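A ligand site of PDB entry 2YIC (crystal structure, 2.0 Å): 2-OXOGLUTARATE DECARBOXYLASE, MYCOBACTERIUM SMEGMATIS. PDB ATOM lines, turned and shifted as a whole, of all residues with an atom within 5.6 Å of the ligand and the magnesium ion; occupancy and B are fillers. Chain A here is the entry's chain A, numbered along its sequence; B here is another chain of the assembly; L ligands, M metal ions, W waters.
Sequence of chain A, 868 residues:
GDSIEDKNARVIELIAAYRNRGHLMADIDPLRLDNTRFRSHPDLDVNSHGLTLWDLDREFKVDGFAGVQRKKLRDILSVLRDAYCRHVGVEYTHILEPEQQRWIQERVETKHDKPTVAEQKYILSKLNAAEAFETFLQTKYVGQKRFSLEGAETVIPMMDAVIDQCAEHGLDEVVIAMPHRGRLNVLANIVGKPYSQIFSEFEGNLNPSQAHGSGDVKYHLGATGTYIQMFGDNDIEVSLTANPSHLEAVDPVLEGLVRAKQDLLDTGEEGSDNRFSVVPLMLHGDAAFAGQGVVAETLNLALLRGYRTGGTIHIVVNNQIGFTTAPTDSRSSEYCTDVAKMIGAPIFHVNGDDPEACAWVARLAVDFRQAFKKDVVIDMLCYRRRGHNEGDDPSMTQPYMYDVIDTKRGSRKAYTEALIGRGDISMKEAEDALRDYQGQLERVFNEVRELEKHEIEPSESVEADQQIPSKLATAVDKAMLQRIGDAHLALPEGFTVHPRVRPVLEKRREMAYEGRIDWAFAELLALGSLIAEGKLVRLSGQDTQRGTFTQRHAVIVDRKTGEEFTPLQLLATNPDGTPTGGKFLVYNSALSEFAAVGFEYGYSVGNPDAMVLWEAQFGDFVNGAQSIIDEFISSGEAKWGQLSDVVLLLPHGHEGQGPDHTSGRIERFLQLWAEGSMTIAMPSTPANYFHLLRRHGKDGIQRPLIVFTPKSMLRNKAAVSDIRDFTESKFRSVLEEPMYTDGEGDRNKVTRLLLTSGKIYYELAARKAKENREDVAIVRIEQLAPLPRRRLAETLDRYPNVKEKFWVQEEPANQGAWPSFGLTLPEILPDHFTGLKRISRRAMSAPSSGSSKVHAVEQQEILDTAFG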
ATOM      1  N   HIS A 180     -36.596  15.731  13.293  1.00  0.00           N
ATOM      2  CA  HIS A 180     -37.596  16.802  13.471  1.00  0.00           C
ATOM      3  C   HIS A 180     -37.437  18.060  12.625  1.00  0.00           C
ATOM      4  O   HIS A 180     -38.447  18.740  12.363  1.00  0.00           O
ATOM      5  CB  HIS A 180     -37.663  17.231  14.947  1.00  0.00           C
ATOM      6  CG  HIS A 180     -36.328  17.595  15.516  1.00  0.00           C
ATOM      7  ND1 HIS A 180     -35.407  16.609  15.875  1.00  0.00           N
ATOM      8  CD2 HIS A 180     -35.798  18.806  15.790  1.00  0.00           C
ATOM      9  CE1 HIS A 180     -34.366  17.260  16.370  1.00  0.00           C
ATOM     10  NE2 HIS A 180     -34.557  18.577  16.362  1.00  0.00           N
ATOM     11  N   ARG A 181     -36.198  18.445  12.248  1.00  0.00           N
ATOM     12  CA  ARG A 181     -36.018  19.695  11.490  1.00  0.00           C
ATOM     13  C   ARG A 181     -36.785  19.706  10.150  1.00  0.00           C
ATOM     14  O   ARG A 181     -36.542  18.869   9.285  1.00  0.00           O
ATOM     15  CB  ARG A 181     -34.531  19.983  11.239  1.00  0.00           C
ATOM     16  CG  ARG A 181     -34.284  21.384  10.734  1.00  0.00           C
ATOM     17  CD  ARG A 181     -32.813  21.741  10.621  1.00  0.00           C
ATOM     18  NE  ARG A 181     -32.085  21.536  11.876  1.00  0.00           N
ATOM     19  CZ  ARG A 181     -32.090  22.382  12.899  1.00  0.00           C
ATOM     20  NH1 ARG A 181     -32.825  23.486  12.854  1.00  0.00           N
ATOM     21  NH2 ARG A 181     -31.382  22.116  13.986  1.00  0.00           N
ATOM     22  N   SER A 245     -36.975  10.727  19.340  1.00  0.00           N
ATOM     23  CA  SER A 245     -36.033  11.841  19.177  1.00  0.00           C
ATOM     24  C   SER A 245     -34.609  11.292  18.944  1.00  0.00           C
ATOM     25  O   SER A 245     -33.740  12.058  18.506  1.00  0.00           O
ATOM     26  CB  SER A 245     -36.055  12.770  20.373  1.00  0.00           C
ATOM     27  OG  SER A 245     -37.307  13.379  20.612  1.00  0.00           O
ATOM     28  N   HIS A 246     -34.371   9.976  19.211  1.00  0.00           N
ATOM     29  CA  HIS A 246     -33.064   9.315  18.992  1.00  0.00           C
ATOM     30  C   HIS A 246     -32.716   9.397  17.512  1.00  0.00           C
ATOM     31  O   HIS A 246     -33.329   8.698  16.695  1.00  0.00           O
ATOM     32  CB  HIS A 246     -33.102   7.850  19.479  1.00  0.00           C
ATOM     33  CG  HIS A 246     -33.175   7.713  20.981  1.00  0.00           C
ATOM     34  ND1 HIS A 246     -34.198   8.327  21.723  1.00  0.00           N
ATOM     35  CD2 HIS A 246     -32.343   7.076  21.836  1.00  0.00           C
ATOM     36  CE1 HIS A 246     -33.953   8.020  22.989  1.00  0.00           C
ATOM     37  NE2 HIS A 246     -32.870   7.254  23.112  1.00  0.00           N
ATOM     38  N   LEU A 247     -31.799  10.304  17.173  1.00  0.00           N
ATOM     39  CA  LEU A 247     -31.388  10.552  15.788  1.00  0.00           C
ATOM     40  C   LEU A 247     -30.803   9.283  15.205  1.00  0.00           C
ATOM     41  O   LEU A 247     -30.015   8.603  15.870  1.00  0.00           O
ATOM     42  CB  LEU A 247     -30.367  11.710  15.728  1.00  0.00           C
ATOM     43  CG  LEU A 247     -30.882  13.069  16.303  1.00  0.00           C
ATOM     44  CD1 LEU A 247     -29.752  14.068  16.426  1.00  0.00           C
ATOM     45  CD2 LEU A 247     -32.040  13.617  15.477  1.00  0.00           C
ATOM     46  N   GLY A 285     -29.136  14.583   9.568  1.00  0.00           N
ATOM     47  CA  GLY A 285     -28.396  15.785   9.935  1.00  0.00           C
ATOM     48  C   GLY A 285     -26.923  15.391   9.780  1.00  0.00           C
ATOM     49  O   GLY A 285     -26.606  14.203   9.878  1.00  0.00           O
ATOM     50  N   ASP A 286     -26.022  16.358   9.568  1.00  0.00           N
ATOM     51  CA  ASP A 286     -24.596  16.055   9.351  1.00  0.00           C
ATOM     52  C   ASP A 286     -23.924  15.441  10.555  1.00  0.00           C
ATOM     53  O   ASP A 286     -23.149  14.510  10.353  1.00  0.00           O
ATOM     54  CB  ASP A 286     -23.818  17.326   8.940  1.00  0.00           C
ATOM     55  CG  ASP A 286     -24.067  18.567   9.804  1.00  0.00           C
ATOM     56  OD1 ASP A 286     -25.228  19.013   9.890  1.00  0.00           O
ATOM     57  OD2 ASP A 286     -23.093  19.126  10.317  1.00  0.00           O
ATOM     58  N   ALA A 287     -24.163  15.974  11.782  1.00  0.00           N
ATOM     59  CA  ALA A 287     -23.466  15.423  12.949  1.00  0.00           C
ATOM     60  C   ALA A 287     -23.940  13.999  13.259  1.00  0.00           C
ATOM     61  O   ALA A 287     -23.099  13.130  13.485  1.00  0.00           O
ATOM     62  CB  ALA A 287     -23.642  16.344  14.169  1.00  0.00           C
ATOM     63  N   ALA A 288     -25.251  13.745  13.223  1.00  0.00           N
ATOM     64  CA  ALA A 288     -25.813  12.418  13.518  1.00  0.00           C
ATOM     65  C   ALA A 288     -25.398  11.355  12.489  1.00  0.00           C
ATOM     66  O   ALA A 288     -25.126  10.216  12.874  1.00  0.00           O
ATOM     67  CB  ALA A 288     -27.316  12.507  13.589  1.00  0.00           C
ATOM     68  N   PHE A 289     -25.368  11.722  11.179  1.00  0.00           N
ATOM     69  CA  PHE A 289     -24.991  10.791  10.119  1.00  0.00           C
ATOM     70  C   PHE A 289     -23.560  10.280  10.312  1.00  0.00           C
ATOM     71  O   PHE A 289     -23.316   9.092  10.106  1.00  0.00           O
ATOM     72  CB  PHE A 289     -25.143  11.479   8.738  1.00  0.00           C
ATOM     73  CG  PHE A 289     -25.176  10.512   7.571  1.00  0.00           C
ATOM     74  CD1 PHE A 289     -26.280   9.690   7.354  1.00  0.00           C
ATOM     75  CD2 PHE A 289     -24.120  10.438   6.673  1.00  0.00           C
ATOM     76  CE1 PHE A 289     -26.315   8.801   6.279  1.00  0.00           C
ATOM     77  CE2 PHE A 289     -24.159   9.550   5.588  1.00  0.00           C
ATOM     78  CZ  PHE A 289     -25.250   8.748   5.390  1.00  0.00           C
ATOM     79  N   GLN A 292     -23.442   8.328  14.554  1.00  0.00           N
ATOM     80  CA  GLN A 292     -24.290   7.205  14.980  1.00  0.00           C
ATOM     81  C   GLN A 292     -23.928   5.914  14.210  1.00  0.00           C
ATOM     82  O   GLN A 292     -24.087   5.837  13.003  1.00  0.00           O
ATOM     83  CB  GLN A 292     -25.786   7.565  14.789  1.00  0.00           C
ATOM     84  CG  GLN A 292     -26.299   8.603  15.832  1.00  0.00           C
ATOM     85  CD  GLN A 292     -26.387   8.012  17.233  1.00  0.00           C
ATOM     86  OE1 GLN A 292     -27.066   7.011  17.456  1.00  0.00           O
ATOM     87  NE2 GLN A 292     -25.678   8.595  18.198  1.00  0.00           N
ATOM     88  N   VAL A 317     -29.147  16.947   5.498  1.00  0.00           N
ATOM     89  CA  VAL A 317     -29.319  18.380   5.641  1.00  0.00           C
ATOM     90  C   VAL A 317     -28.067  18.855   6.377  1.00  0.00           C
ATOM     91  O   VAL A 317     -27.985  18.774   7.612  1.00  0.00           O
ATOM     92  CB  VAL A 317     -30.627  18.726   6.352  1.00  0.00           C
ATOM     93  CG1 VAL A 317     -30.765  20.252   6.543  1.00  0.00           C
ATOM     94  CG2 VAL A 317     -31.815  18.155   5.597  1.00  0.00           C
ATOM     95  N   ASN A 318     -27.041  19.223   5.596  1.00  0.00           N
ATOM     96  CA  ASN A 318     -25.760  19.553   6.172  1.00  0.00           C
ATOM     97  C   ASN A 318     -25.631  21.055   6.444  1.00  0.00           C
ATOM     98  O   ASN A 318     -25.109  21.792   5.619  1.00  0.00           O
ATOM     99  CB  ASN A 318     -24.641  19.040   5.252  1.00  0.00           C
ATOM    100  CG  ASN A 318     -23.247  19.258   5.778  1.00  0.00           C
ATOM    101  OD1 ASN A 318     -23.047  19.787   6.874  1.00  0.00           O
ATOM    102  ND2 ASN A 318     -22.270  18.914   4.965  1.00  0.00           N
ATOM    103  N   ASN A 319     -26.054  21.485   7.656  1.00  0.00           N
ATOM    104  CA  ASN A 319     -25.986  22.914   8.042  1.00  0.00           C
ATOM    105  C   ASN A 319     -24.640  23.231   8.732  1.00  0.00           C
ATOM    106  O   ASN A 319     -24.485  24.305   9.327  1.00  0.00           O
ATOM    107  CB  ASN A 319     -27.137  23.315   8.902  1.00  0.00           C
ATOM    108  CG  ASN A 319     -27.433  22.363  10.044  1.00  0.00           C
ATOM    109  OD1 ASN A 319     -26.563  21.618  10.514  1.00  0.00           O
ATOM    110  ND2 ASN A 319     -28.669  22.389  10.514  1.00  0.00           N
ATOM    111  N   GLN A 320     -23.693  22.264   8.677  1.00  0.00           N
ATOM    112  CA  GLN A 320     -22.277  22.399   9.103  1.00  0.00           C
ATOM    113  C   GLN A 320     -22.144  22.749  10.585  1.00  0.00           C
ATOM    114  O   GLN A 320     -21.210  23.440  10.994  1.00  0.00           O
ATOM    115  CB  GLN A 320     -21.582  23.455   8.216  1.00  0.00           C
ATOM    116  CG  GLN A 320     -21.925  23.323   6.688  1.00  0.00           C
ATOM    117  CD  GLN A 320     -21.302  24.427   5.852  1.00  0.00           C
ATOM    118  OE1 GLN A 320     -20.088  24.551   5.786  1.00  0.00           O
ATOM    119  NE2 GLN A 320     -22.105  25.312   5.250  1.00  0.00           N
ATOM    120  N   ILE A 321     -23.089  22.240  11.390  1.00  0.00           N
ATOM    121  CA  ILE A 321     -23.148  22.425  12.846  1.00  0.00           C
ATOM    122  C   ILE A 321     -24.006  21.324  13.448  1.00  0.00           C
ATOM    123  O   ILE A 321     -24.937  20.827  12.796  1.00  0.00           O
ATOM    124  CB  ILE A 321     -23.683  23.864  13.210  1.00  0.00           C
ATOM    125  CG1 ILE A 321     -23.395  24.231  14.678  1.00  0.00           C
ATOM    126  CG2 ILE A 321     -25.166  24.078  12.779  1.00  0.00           C
ATOM    127  CD1 ILE A 321     -23.657  25.754  15.043  1.00  0.00           C
ATOM    128  N   GLY A 322     -23.678  20.948  14.679  1.00  0.00           N
ATOM    129  CA  GLY A 322     -24.430  19.954  15.421  1.00  0.00           C
ATOM    130  C   GLY A 322     -24.735  20.511  16.791  1.00  0.00           C
ATOM    131  O   GLY A 322     -23.935  20.334  17.711  1.00  0.00           O
ATOM    132  N   PHE A 323     -25.830  21.304  16.878  1.00  0.00           N
ATOM    133  CA  PHE A 323     -26.218  22.033  18.087  1.00  0.00           C
ATOM    134  C   PHE A 323     -25.148  23.128  18.304  1.00  0.00           C
ATOM    135  O   PHE A 323     -25.259  24.138  17.647  1.00  0.00           O
ATOM    136  CB  PHE A 323     -26.457  21.093  19.306  1.00  0.00           C
ATOM    137  CG  PHE A 323     -27.140  21.625  20.547  1.00  0.00           C
ATOM    138  CD1 PHE A 323     -27.236  22.987  20.786  1.00  0.00           C
ATOM    139  CD2 PHE A 323     -27.660  20.756  21.490  1.00  0.00           C
ATOM    140  CE1 PHE A 323     -27.826  23.467  21.967  1.00  0.00           C
ATOM    141  CE2 PHE A 323     -28.238  21.228  22.667  1.00  0.00           C
ATOM    142  CZ  PHE A 323     -28.339  22.583  22.885  1.00  0.00           C
ATOM    143  N   ARG A 384     -27.969  26.881   9.365  1.00  0.00           N
ATOM    144  CA  ARG A 384     -29.046  26.937  10.345  1.00  0.00           C
ATOM    145  C   ARG A 384     -29.177  28.381  10.741  1.00  0.00           C
ATOM    146  O   ARG A 384     -28.300  28.904  11.415  1.00  0.00           O
ATOM    147  CB  ARG A 384     -28.712  25.988  11.532  1.00  0.00           C
ATOM    148  CG  ARG A 384     -29.850  25.815  12.560  1.00  0.00           C
ATOM    149  CD  ARG A 384     -29.338  25.250  13.880  1.00  0.00           C
ATOM    150  NE  ARG A 384     -28.559  26.278  14.562  1.00  0.00           N
ATOM    151  CZ  ARG A 384     -27.623  26.049  15.483  1.00  0.00           C
ATOM    152  NH1 ARG A 384     -27.336  24.801  15.855  1.00  0.00           N
ATOM    153  NH2 ARG A 384     -26.945  27.047  16.008  1.00  0.00           N
ATOM    154  N   HIS A 388     -29.926  26.801  18.043  1.00  0.00           N
ATOM    155  CA  HIS A 388     -30.480  25.448  18.120  1.00  0.00           C
ATOM    156  C   HIS A 388     -31.890  25.416  18.703  1.00  0.00           C
ATOM    157  O   HIS A 388     -32.684  24.559  18.305  1.00  0.00           O
ATOM    158  CB  HIS A 388     -29.604  24.517  18.927  1.00  0.00           C
ATOM    159  CG  HIS A 388     -29.794  23.082  18.532  1.00  0.00           C
ATOM    160  ND1 HIS A 388     -29.489  22.626  17.244  1.00  0.00           N
ATOM    161  CD2 HIS A 388     -30.290  22.046  19.251  1.00  0.00           C
ATOM    162  CE1 HIS A 388     -29.796  21.342  17.235  1.00  0.00           C
ATOM    163  NE2 HIS A 388     -30.277  20.943  18.421  1.00  0.00           N
ATOM    164  N   GLN B 542     -21.988  15.571  24.647  1.00  0.00           N
ATOM    165  CA  GLN B 542     -22.533  16.410  23.583  1.00  0.00           C
ATOM    166  C   GLN B 542     -22.790  17.832  24.067  1.00  0.00           C
ATOM    167  O   GLN B 542     -23.483  18.035  25.075  1.00  0.00           O
ATOM    168  CB  GLN B 542     -23.786  15.763  23.017  1.00  0.00           C
ATOM    169  CG  GLN B 542     -23.457  14.556  22.126  1.00  0.00           C
ATOM    170  CD  GLN B 542     -24.582  13.553  22.108  1.00  0.00           C
ATOM    171  OE1 GLN B 542     -25.759  13.889  22.342  1.00  0.00           O
ATOM    172  NE2 GLN B 542     -24.253  12.277  21.853  1.00  0.00           N
ATOM    173  N   ASP B 543     -22.107  18.806  23.424  1.00  0.00           N
ATOM    174  CA  ASP B 543     -22.204  20.242  23.722  1.00  0.00           C
ATOM    175  C   ASP B 543     -21.835  20.555  25.189  1.00  0.00           C
ATOM    176  O   ASP B 543     -22.258  21.588  25.728  1.00  0.00           O
ATOM    177  CB  ASP B 543     -23.582  20.731  23.346  1.00  0.00           C
ATOM    178  CG  ASP B 543     -23.862  20.385  21.887  1.00  0.00           C
ATOM    179  OD1 ASP B 543     -23.230  21.011  21.003  1.00  0.00           O
ATOM    180  OD2 ASP B 543     -24.574  19.388  21.641  1.00  0.00           O
ATOM    181  N   LEU B 591     -21.404  13.002  17.946  1.00  0.00           N
ATOM    182  CA  LEU B 591     -22.771  12.615  18.210  1.00  0.00           C
ATOM    183  C   LEU B 591     -22.858  11.098  18.295  1.00  0.00           C
ATOM    184  O   LEU B 591     -23.373  10.423  17.401  1.00  0.00           O
ATOM    185  CB  LEU B 591     -23.721  13.185  17.148  1.00  0.00           C
ATOM    186  CG  LEU B 591     -25.095  13.598  17.664  1.00  0.00           C
ATOM    187  CD1 LEU B 591     -25.762  14.478  16.690  1.00  0.00           C
ATOM    188  CD2 LEU B 591     -25.984  12.387  17.992  1.00  0.00           C
ATOM    189  N   GLU B 593     -23.095   7.818  21.473  1.00  0.00           N
ATOM    190  CA  GLU B 593     -23.255   7.439  22.873  1.00  0.00           C
ATOM    191  C   GLU B 593     -22.413   6.204  23.116  1.00  0.00           C
ATOM    192  O   GLU B 593     -21.553   6.201  24.005  1.00  0.00           O
ATOM    193  CB  GLU B 593     -24.761   7.211  23.243  1.00  0.00           C
ATOM    194  CG  GLU B 593     -25.527   8.520  23.373  1.00  0.00           C
ATOM    195  CD  GLU B 593     -26.012   9.139  22.079  1.00  0.00           C
ATOM    196  OE1 GLU B 593     -26.231   8.400  21.103  1.00  0.00           O
ATOM    197  OE2 GLU B 593     -26.198  10.376  22.053  1.00  0.00           O
ATOM    198  N   GLN B 617     -26.643  14.183  26.611  1.00  0.00           N
ATOM    199  CA  GLN B 617     -27.327  15.447  26.344  1.00  0.00           C
ATOM    200  C   GLN B 617     -28.580  15.518  27.240  1.00  0.00           C
ATOM    201  O   GLN B 617     -28.869  16.532  27.899  1.00  0.00           O
ATOM    202  CB  GLN B 617     -27.662  15.552  24.841  1.00  0.00           C
ATOM    203  CG  GLN B 617     -28.384  16.838  24.514  1.00  0.00           C
ATOM    204  CD  GLN B 617     -27.657  17.625  23.468  1.00  0.00           C
ATOM    205  OE1 GLN B 617     -28.072  17.664  22.342  1.00  0.00           O
ATOM    206  NE2 GLN B 617     -26.615  18.325  23.849  1.00  0.00           N
ATOM    207  N   PHE B 621     -30.886   9.356  26.139  1.00  0.00           N
ATOM    208  CA  PHE B 621     -30.057   8.900  25.031  1.00  0.00           C
ATOM    209  C   PHE B 621     -29.001   7.936  25.448  1.00  0.00           C
ATOM    210  O   PHE B 621     -28.424   7.270  24.579  1.00  0.00           O
ATOM    211  CB  PHE B 621     -29.443  10.111  24.291  1.00  0.00           C
ATOM    212  CG  PHE B 621     -30.532  11.003  23.752  1.00  0.00           C
ATOM    213  CD1 PHE B 621     -31.469  10.524  22.847  1.00  0.00           C
ATOM    214  CD2 PHE B 621     -30.660  12.315  24.203  1.00  0.00           C
ATOM    215  CE1 PHE B 621     -32.497  11.335  22.386  1.00  0.00           C
ATOM    216  CE2 PHE B 621     -31.703  13.134  23.738  1.00  0.00           C
ATOM    217  CZ  PHE B 621     -32.616  12.636  22.854  1.00  0.00           C
ATOM    218  N   HIS B 661     -37.101  13.156  26.546  1.00  0.00           N
ATOM    219  CA  HIS B 661     -36.444  14.292  27.217  1.00  0.00           C
ATOM    220  C   HIS B 661     -36.916  14.323  28.654  1.00  0.00           C
ATOM    221  O   HIS B 661     -37.128  15.398  29.236  1.00  0.00           O
ATOM    222  CB  HIS B 661     -36.746  15.595  26.470  1.00  0.00           C
ATOM    223  CG  HIS B 661     -36.181  15.609  25.087  1.00  0.00           C
ATOM    224  ND1 HIS B 661     -36.894  15.112  24.022  1.00  0.00           N
ATOM    225  CD2 HIS B 661     -34.951  15.977  24.669  1.00  0.00           C
ATOM    226  CE1 HIS B 661     -36.107  15.218  22.970  1.00  0.00           C
ATOM    227  NE2 HIS B 661     -34.918  15.739  23.315  1.00  0.00           N
HETATM  228  N1  LIG L   1     -28.308  11.521  20.713  1.00  0.00           N
HETATM  229  C1  LIG L   1     -29.297  10.964  20.035  1.00  0.00           C
HETATM  230  C2  LIG L   1     -29.185   9.528  19.625  1.00  0.00           C
HETATM  231  N2  LIG L   1     -30.368  11.670  19.647  1.00  0.00           N
HETATM  232  C3  LIG L   1     -30.497  12.967  19.989  1.00  0.00           C
HETATM  233  N3  LIG L   1     -31.656  13.634  19.664  1.00  0.00           N
HETATM  234  C4  LIG L   1     -29.461  13.602  20.709  1.00  0.00           C
HETATM  235  C5  LIG L   1     -28.376  12.820  21.075  1.00  0.00           C
HETATM  236  C6  LIG L   1     -29.550  15.066  21.113  1.00  0.00           C
HETATM  237  N4  LIG L   1     -29.451  16.023  19.979  1.00  0.00           N
HETATM  238  C7  LIG L   1     -30.514  16.635  19.539  1.00  0.00           C
HETATM  239  S1  LIG L   1     -30.138  17.655  18.212  1.00  0.00           S
HETATM  240  C8  LIG L   1     -28.444  17.266  18.349  1.00  0.00           C
HETATM  241  C9  LIG L   1     -28.320  16.351  19.339  1.00  0.00           C
HETATM  242  C10 LIG L   1     -26.931  15.897  19.712  1.00  0.00           C
HETATM  243  C11 LIG L   1     -27.422  17.858  17.393  1.00  0.00           C
HETATM  244  C12 LIG L   1     -27.852  17.321  16.008  1.00  0.00           C
HETATM  245  O1  LIG L   1     -26.971  17.709  14.951  1.00  0.00           O
HETATM  246  P1  LIG L   1     -27.275  17.336  13.434  1.00  0.00           P
HETATM  247  O2  LIG L   1     -27.293  15.838  13.292  1.00  0.00           O
HETATM  248  O3  LIG L   1     -26.162  17.986  12.503  1.00  0.00           O
HETATM  249  O4  LIG L   1     -28.736  17.975  13.100  1.00  0.00           O
HETATM  250  P2  LIG L   1     -29.216  19.423  13.092  1.00  0.00           P
HETATM  251  O5  LIG L   1     -29.899  19.800  14.460  1.00  0.00           O
HETATM  252  O6  LIG L   1     -28.033  20.319  12.814  1.00  0.00           O
HETATM  253  O7  LIG L   1     -30.220  19.531  11.846  1.00  0.00           O
HETATM  254 MG    MG M   1     -26.348  19.746  11.520  1.00  0.00          MG
HETATM  255  O   HOH W   1     -32.173  19.640  15.920  1.00  0.00           O
HETATM  256  O   HOH W   2     -31.247  17.141  11.480  1.00  0.00           O
HETATM  257  O   HOH W   3     -27.871  19.151  10.225  1.00  0.00           O
HETATM  258  O   HOH W   4     -24.118  17.912  19.328  1.00  0.00           O
HETATM  259  O   HOH W   5     -30.085  14.973  12.788  1.00  0.00           O
HETATM  260  O   HOH W   6     -27.857  22.102  14.959  1.00  0.00           O
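Of the 27 residues printed, 3 come within 4 Å of the magnesium ion.
The magnesium ion is bound by an oxygen (O3) of the ligand (2.0 Å), water W3 (2.1 Å), the side-chain carboxylate (OD1) of Asp 286 (2.1 Å), the side-chain amide oxygen (OD1) of Asn 319 (2.1 Å), the backbone carbonyl oxygen (O) of Ile 321 (2.2 Å) and an oxygen (O6) of the ligand (2.2 Å). The magnesium ion has six donor atoms within binding distance.
A nitrogen (N4) of the ligand sits close to the side-chain amide oxygen (OE1) of Gln 617 of chain B, at 3.2 Å. Merely in contact with the ligand: Gln 542 of chain B (3.1 Å), Gly 322 (3.4 Å), Phe 621 of chain B (3.5 Å), Gly 285 (3.5 Å), Leu 591 of chain B (3.5 Å), His 246 (3.6 Å), Phe 323 (3.8 Å) and Gln 292 (3.9 Å). Hydrophobic or aromatic side chains that line the ligand: Leu 247, Ala 287, Ala 288, Phe 323, His 388, Leu 591 of chain B and Phe 621 of chain B. Of the 27 residues printed, 19 come within 4 Å of the ligand. The nearest printed residue that does not touch the ligand is His 180 (4.6 Å).
The side-chain carboxylate (OE2) of Glu 593 of chain B is in hydrogen-bond range of a nitrogen (N1) of the ligand, 2.7 Å away. An oxygen (O2) of the ligand lies within hydrogen-bond range of the backbone NH of Ala 288 (2.9 Å). O of Ser 245 lies within hydrogen-bond range of N3 of the ligand. O7 of the ligand is in salt-bridge range of NE of Arg 181 (2.7 Å). O3 of the ligand sits close to N of Asp 286 (3.4 Å). The backbone NH (N) of Leu 247 sits at hydrogen-bond distance from a nitrogen (N2) of the ligand. N of Ala 287 sits at hydrogen-bond distance from O2 of the ligand, at 3.5 Å. A ring nitrogen (NE2) of His 388 sits close to a sulfur (S1) of the ligand (3.3 Å).
Water W3 lies within hydrogen-bond range of O of Val 317 (2.6 Å), O7 of the ligand (2.9 Å), ND2 of Asn 319 (3.3 Å) and N of Asp 286 (3.4 Å). Water W1 lies within hydrogen-bond range of a ring nitrogen (NE2) of His 180 (2.6 Å), an oxygen (O5) of the ligand (2.7 Å), the guanidinium group (NH2) of Arg 181 (3.2 Å) and a ring nitrogen (NE2) of His 388 (3.4 Å). Water W6 lies within hydrogen-bond range of a ring nitrogen (ND1) of His 388 (2.9 Å), the guanidinium group (NH1) of Arg 384 (2.9 Å), the backbone NH (N) of Phe 323 (2.9 Å) and an oxygen (O5) of the ligand (3.1 Å). Water W5 bridges an oxygen (O2) of the ligand and the backbone NH (N) of Gly 285. Water W4 lies within hydrogen-bond range of the side-chain carboxylate of Asp 543 of chain B (2.8 Å) and the backbone carbonyl oxygen of Gly 322 (2.9 Å).
The side-chain carboxylate (OE2) of Glu 593 of chain B lies within hydrogen-bond range of the side-chain amide nitrogen (NE2) of Gln 542 of chain B. The side-chain carboxylate of Glu 593 of chain B lies within hydrogen-bond range of the side-chain amide nitrogen of Gln 292 (3.0 Å). O of Gln 542 of chain B sits at hydrogen-bond distance from NE2 of Gln 617 of chain B (3.4 Å). The backbone carbonyl oxygen of Leu 591 of chain B is in hydrogen-bond range of the side-chain amide nitrogen of Gln 292. NE2 of Gln 617 of chain B is in hydrogen-bond range of OD2 of Asp 543 of chain B (3.2 Å). A ring nitrogen (ND1) of His 388 lies within hydrogen-bond range of the guanidinium group (NH1) of Arg 384, 3.4 Å away. The backbone carbonyl oxygen of Phe 323 sits at hydrogen-bond distance from the guanidinium group of Arg 384 (2.8 Å).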
